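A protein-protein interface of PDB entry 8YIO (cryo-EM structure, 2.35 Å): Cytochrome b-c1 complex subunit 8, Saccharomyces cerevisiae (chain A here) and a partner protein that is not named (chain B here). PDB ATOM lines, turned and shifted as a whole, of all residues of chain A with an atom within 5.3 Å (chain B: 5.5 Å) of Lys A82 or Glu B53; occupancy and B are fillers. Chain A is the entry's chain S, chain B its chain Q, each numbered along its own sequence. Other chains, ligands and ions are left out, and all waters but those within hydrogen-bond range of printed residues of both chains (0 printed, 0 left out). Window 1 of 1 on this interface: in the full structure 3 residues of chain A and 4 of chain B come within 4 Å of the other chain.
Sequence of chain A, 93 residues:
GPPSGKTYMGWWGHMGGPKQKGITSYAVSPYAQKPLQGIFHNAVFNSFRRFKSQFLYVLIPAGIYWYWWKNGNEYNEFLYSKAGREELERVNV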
ATOM      1  N   TYR A  80      15.786  -8.027   7.660  1.00  0.00           N
ATOM      2  CA  TYR A  80      16.082  -9.038   6.656  1.00  0.00           C
ATOM      3  C   TYR A  80      17.127  -8.580   5.650  1.00  0.00           C
ATOM      4  O   TYR A  80      17.299  -9.223   4.612  1.00  0.00           O
ATOM      5  CB  TYR A  80      14.792  -9.464   5.950  1.00  0.00           C
ATOM      6  CG  TYR A  80      13.958 -10.382   6.809  1.00  0.00           C
ATOM      7  CD1 TYR A  80      14.217 -11.744   6.854  1.00  0.00           C
ATOM      8  CD2 TYR A  80      12.936  -9.883   7.607  1.00  0.00           C
ATOM      9  CE1 TYR A  80      13.471 -12.586   7.651  1.00  0.00           C
ATOM     10  CE2 TYR A  80      12.185 -10.717   8.409  1.00  0.00           C
ATOM     11  CZ  TYR A  80      12.457 -12.066   8.425  1.00  0.00           C
ATOM     12  OH  TYR A  80      11.713 -12.900   9.218  1.00  0.00           O
ATOM     13  N   SER A  81      17.831  -7.491   5.936  1.00  0.00           N
ATOM     14  CA  SER A  81      18.950  -7.049   5.120  1.00  0.00           C
ATOM     15  C   SER A  81      20.247  -7.614   5.699  1.00  0.00           C
ATOM     16  O   SER A  81      20.233  -8.436   6.619  1.00  0.00           O
ATOM     17  CB  SER A  81      18.967  -5.525   5.034  1.00  0.00           C
ATOM     18  OG  SER A  81      19.650  -4.959   6.138  1.00  0.00           O
ATOM     19  N   LYS A  82      21.387  -7.186   5.154  1.00  0.00           N
ATOM     20  CA  LYS A  82      22.673  -7.660   5.661  1.00  0.00           C
ATOM     21  C   LYS A  82      23.031  -6.993   6.979  1.00  0.00           C
ATOM     22  O   LYS A  82      23.599  -7.635   7.870  1.00  0.00           O
ATOM     23  CB  LYS A  82      23.775  -7.403   4.636  1.00  0.00           C
ATOM     24  CG  LYS A  82      23.863  -8.429   3.539  1.00  0.00           C
ATOM     25  CD  LYS A  82      24.597  -7.863   2.341  1.00  0.00           C
ATOM     26  CE  LYS A  82      26.090  -7.966   2.517  1.00  0.00           C
ATOM     27  NZ  LYS A  82      26.476  -9.390   2.626  1.00  0.00           N
ATOM     28  N   ALA A  83      22.719  -5.704   7.115  1.00  0.00           N
ATOM     29  CA  ALA A  83      23.092  -4.952   8.306  1.00  0.00           C
ATOM     30  C   ALA A  83      22.279  -5.344   9.531  1.00  0.00           C
ATOM     31  O   ALA A  83      22.753  -5.158  10.656  1.00  0.00           O
ATOM     32  CB  ALA A  83      22.946  -3.455   8.043  1.00  0.00           C
ATOM     33  N   GLY A  84      21.076  -5.877   9.343  1.00  0.00           N
ATOM     34  CA  GLY A  84      20.241  -6.251  10.463  1.00  0.00           C
ATOM     35  C   GLY A  84      20.235  -7.738  10.723  1.00  0.00           C
ATOM     36  O   GLY A  84      19.269  -8.272  11.273  1.00  0.00           O
ATOM     37  N   ARG A  85      21.311  -8.421  10.333  1.00  0.00           N
ATOM     38  CA  ARG A  85      21.359  -9.867  10.512  1.00  0.00           C
ATOM     39  C   ARG A  85      21.577 -10.254  11.971  1.00  0.00           C
ATOM     40  O   ARG A  85      21.002 -11.242  12.435  1.00  0.00           O
ATOM     41  CB  ARG A  85      22.452 -10.473   9.631  1.00  0.00           C
ATOM     42  CG  ARG A  85      22.396 -11.985   9.519  1.00  0.00           C
ATOM     43  CD  ARG A  85      23.647 -12.530   8.869  1.00  0.00           C
ATOM     44  NE  ARG A  85      24.849 -11.946   9.451  1.00  0.00           N
ATOM     45  CZ  ARG A  85      25.528 -12.475  10.464  1.00  0.00           C
ATOM     46  NH1 ARG A  85      25.132 -13.616  11.012  1.00  0.00           N
ATOM     47  NH2 ARG A  85      26.607 -11.862  10.925  1.00  0.00           N
ATOM     48  N   GLU B  49      29.228 -14.952   3.483  1.00  0.00           N
ATOM     49  CA  GLU B  49      28.766 -13.733   2.840  1.00  0.00           C
ATOM     50  C   GLU B  49      28.603 -13.927   1.334  1.00  0.00           C
ATOM     51  O   GLU B  49      29.387 -14.628   0.690  1.00  0.00           O
ATOM     52  CB  GLU B  49      29.754 -12.598   3.129  1.00  0.00           C
ATOM     53  CG  GLU B  49      29.837 -12.141   4.570  1.00  0.00           C
ATOM     54  CD  GLU B  49      30.887 -11.069   4.778  1.00  0.00           C
ATOM     55  OE1 GLU B  49      31.675 -10.820   3.844  1.00  0.00           O
ATOM     56  OE2 GLU B  49      30.923 -10.473   5.875  1.00  0.00           O
ATOM     57  N   ASP B  50      27.565 -13.299   0.783  1.00  0.00           N
ATOM     58  CA  ASP B  50      27.337 -13.221  -0.652  1.00  0.00           C
ATOM     59  C   ASP B  50      27.488 -11.769  -1.087  1.00  0.00           C
ATOM     60  O   ASP B  50      27.742 -10.879  -0.272  1.00  0.00           O
ATOM     61  CB  ASP B  50      25.944 -13.740  -1.026  1.00  0.00           C
ATOM     62  CG  ASP B  50      25.828 -15.238  -0.903  1.00  0.00           C
ATOM     63  OD1 ASP B  50      26.874 -15.915  -0.886  1.00  0.00           O
ATOM     64  OD2 ASP B  50      24.687 -15.740  -0.831  1.00  0.00           O
ATOM     65  N   CYS B  51      27.385 -11.508  -2.372  1.00  0.00           N
ATOM     66  CA  CYS B  51      27.288 -10.158  -2.908  1.00  0.00           C
ATOM     67  C   CYS B  51      25.950  -9.991  -3.622  1.00  0.00           C
ATOM     68  O   CYS B  51      25.971  -9.223  -4.502  1.00  0.00           O
ATOM     69  CB  CYS B  51      28.296  -9.957  -3.998  1.00  0.00           C
ATOM     70  SG  CYS B  51      29.991 -10.434  -3.585  1.00  0.00           S
ATOM     71  N   VAL B  52      24.838 -10.617  -3.180  1.00  0.00           N
ATOM     72  CA  VAL B  52      23.544 -10.559  -3.852  1.00  0.00           C
ATOM     73  C   VAL B  52      22.935  -9.167  -3.729  1.00  0.00           C
ATOM     74  O   VAL B  52      22.386  -8.629  -4.699  1.00  0.00           O
ATOM     75  CB  VAL B  52      22.612 -11.649  -3.287  1.00  0.00           C
ATOM     76  CG1 VAL B  52      21.227 -11.572  -3.907  1.00  0.00           C
ATOM     77  CG2 VAL B  52      23.207 -13.017  -3.518  1.00  0.00           C
ATOM     78  N   GLU B  53      23.047  -8.548  -2.550  1.00  0.00           N
ATOM     79  CA  GLU B  53      22.462  -7.226  -2.352  1.00  0.00           C
ATOM     80  C   GLU B  53      23.246  -6.137  -3.072  1.00  0.00           C
ATOM     81  O   GLU B  53      22.666  -5.124  -3.473  1.00  0.00           O
ATOM     82  CB  GLU B  53      22.354  -6.915  -0.860  1.00  0.00           C
ATOM     83  CG  GLU B  53      21.446  -7.873  -0.112  1.00  0.00           C
ATOM     84  CD  GLU B  53      21.218  -7.470   1.331  1.00  0.00           C
ATOM     85  OE1 GLU B  53      21.474  -6.296   1.673  1.00  0.00           O
ATOM     86  OE2 GLU B  53      20.770  -8.328   2.121  1.00  0.00           O
ATOM     87  N   GLU B  54      24.555  -6.322  -3.247  1.00  0.00           N
ATOM     88  CA  GLU B  54      25.313  -5.404  -4.089  1.00  0.00           C
ATOM     89  C   GLU B  54      24.977  -5.603  -5.561  1.00  0.00           C
ATOM     90  O   GLU B  54      24.953  -4.634  -6.327  1.00  0.00           O
ATOM     91  CB  GLU B  54      26.811  -5.586  -3.854  1.00  0.00           C
ATOM     92  CG  GLU B  54      27.313  -5.000  -2.547  1.00  0.00           C
ATOM     93  CD  GLU B  54      27.181  -5.962  -1.383  1.00  0.00           C
ATOM     94  OE1 GLU B  54      27.453  -5.552  -0.237  1.00  0.00           O
ATOM     95  OE2 GLU B  54      26.804  -7.127  -1.611  1.00  0.00           O
ATOM     96  N   PHE B  55      24.713  -6.846  -5.968  1.00  0.00           N
ATOM     97  CA  PHE B  55      24.294  -7.116  -7.338  1.00  0.00           C
ATOM     98  C   PHE B  55      22.877  -6.612  -7.592  1.00  0.00           C
ATOM     99  O   PHE B  55      22.565  -6.154  -8.696  1.00  0.00           O
ATOM    100  CB  PHE B  55      24.401  -8.616  -7.620  1.00  0.00           C
ATOM    101  CG  PHE B  55      23.944  -9.019  -8.992  1.00  0.00           C
ATOM    102  CD1 PHE B  55      24.739  -8.780 -10.100  1.00  0.00           C
ATOM    103  CD2 PHE B  55      22.725  -9.657  -9.170  1.00  0.00           C
ATOM    104  CE1 PHE B  55      24.324  -9.157 -11.361  1.00  0.00           C
ATOM    105  CE2 PHE B  55      22.302 -10.033 -10.430  1.00  0.00           C
ATOM    106  CZ  PHE B  55      23.103  -9.784 -11.526  1.00  0.00           C
ATOM    107  N   PHE B  56      22.010  -6.682  -6.578  1.00  0.00           N
ATOM    108  CA  PHE B  56      20.634  -6.218  -6.729  1.00  0.00           C
ATOM    109  C   PHE B  56      20.555  -4.700  -6.833  1.00  0.00           C
ATOM    110  O   PHE B  56      19.633  -4.174  -7.466  1.00  0.00           O
ATOM    111  CB  PHE B  56      19.779  -6.697  -5.555  1.00  0.00           C
ATOM    112  CG  PHE B  56      19.081  -8.007  -5.793  1.00  0.00           C
ATOM    113  CD1 PHE B  56      19.666  -9.002  -6.558  1.00  0.00           C
ATOM    114  CD2 PHE B  56      17.833  -8.246  -5.236  1.00  0.00           C
ATOM    115  CE1 PHE B  56      19.017 -10.207  -6.767  1.00  0.00           C
ATOM    116  CE2 PHE B  56      17.182  -9.447  -5.441  1.00  0.00           C
ATOM    117  CZ  PHE B  56      17.773 -10.426  -6.206  1.00  0.00           C
ATOM    118  N   HIS B  57      21.497  -3.982  -6.214  1.00  0.00           N
ATOM    119  CA  HIS B  57      21.472  -2.524  -6.265  1.00  0.00           C
ATOM    120  C   HIS B  57      21.878  -2.009  -7.640  1.00  0.00           C
ATOM    121  O   HIS B  57      21.347  -0.997  -8.111  1.00  0.00           O
ATOM    122  CB  HIS B  57      22.391  -1.942  -5.191  1.00  0.00           C
ATOM    123  CG  HIS B  57      21.801  -1.949  -3.816  1.00  0.00           C
ATOM    124  ND1 HIS B  57      22.573  -1.888  -2.676  1.00  0.00           N
ATOM    125  CD2 HIS B  57      20.516  -2.013  -3.397  1.00  0.00           C
ATOM    126  CE1 HIS B  57      21.788  -1.913  -1.613  1.00  0.00           C
ATOM    127  NE2 HIS B  57      20.535  -1.988  -2.024  1.00  0.00           N
ATOM    128  N   LEU B  58      22.820  -2.687  -8.294  1.00  0.00           N
ATOM    129  CA  LEU B  58      23.225  -2.287  -9.636  1.00  0.00           C
ATOM    130  C   LEU B  58      22.160  -2.650 -10.663  1.00  0.00           C
ATOM    131  O   LEU B  58      21.916  -1.889 -11.605  1.00  0.00           O
ATOM    132  CB  LEU B  58      24.567  -2.929  -9.985  1.00  0.00           C
ATOM    133  CG  LEU B  58      25.088  -2.823 -11.420  1.00  0.00           C
ATOM    134  CD1 LEU B  58      25.300  -1.373 -11.825  1.00  0.00           C
ATOM    135  CD2 LEU B  58      26.371  -3.616 -11.570  1.00  0.00           C
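The backbone carbonyl oxygen (O) of Asp B50 is in hydrogen-bond range of the side-chain amino group (NZ) of Lys A82 (3.5 Å). N of Lys A82 is in hydrogen-bond range of OE2 of Glu B53, 3.3 Å away.
ND1 of His B57 lies close to O of Glu B53 (3.3 Å). OG of Ser A81 sits at hydrogen-bond distance from N of Ala A83, 3.3 Å away.
Among the printed residues, merely in contact across the chains: Ser A81 with Glu B53 (3.7 Å) and Lys A82 with Glu B54 (3.9 Å).
Of chain B, only Asp B50 (3.5 Å), Glu B53 (3.3 Å) and Glu B54 (3.9 Å) come within 4 Å of Lys A82. Glu B53 touches two residues of chain A. Printed residues of chain A within 4 Å of Asp B50: Lys A82 (3.5 Å). Printed residues of chain B within 4 Å of Ser A81: Glu B53 (3.7 Å). Printed residues of chain A within 4 Å of Glu B54: Lys A82 (3.9 Å). The nearest residue of chain B that does not touch Lys A82 is Glu B49 (4.6 Å). The nearest printed residue of chain A that does not touch Glu B54 is Ala A83 (8.7 Å).
Of the 6 printed residues of chain A, 2 touch a printed residue of chain B. Printed residues of chain A that touch a printed residue of chain B: Ser A81 and Lys A82. Along chain A the printed residues that touch a printed residue of chain B span positions 81 to 82. Printed residues of chain B that touch a printed residue of chain A: Asp B50, Glu B53 and Glu B54. Among the printed residues, 4 pairs touch across the chains.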
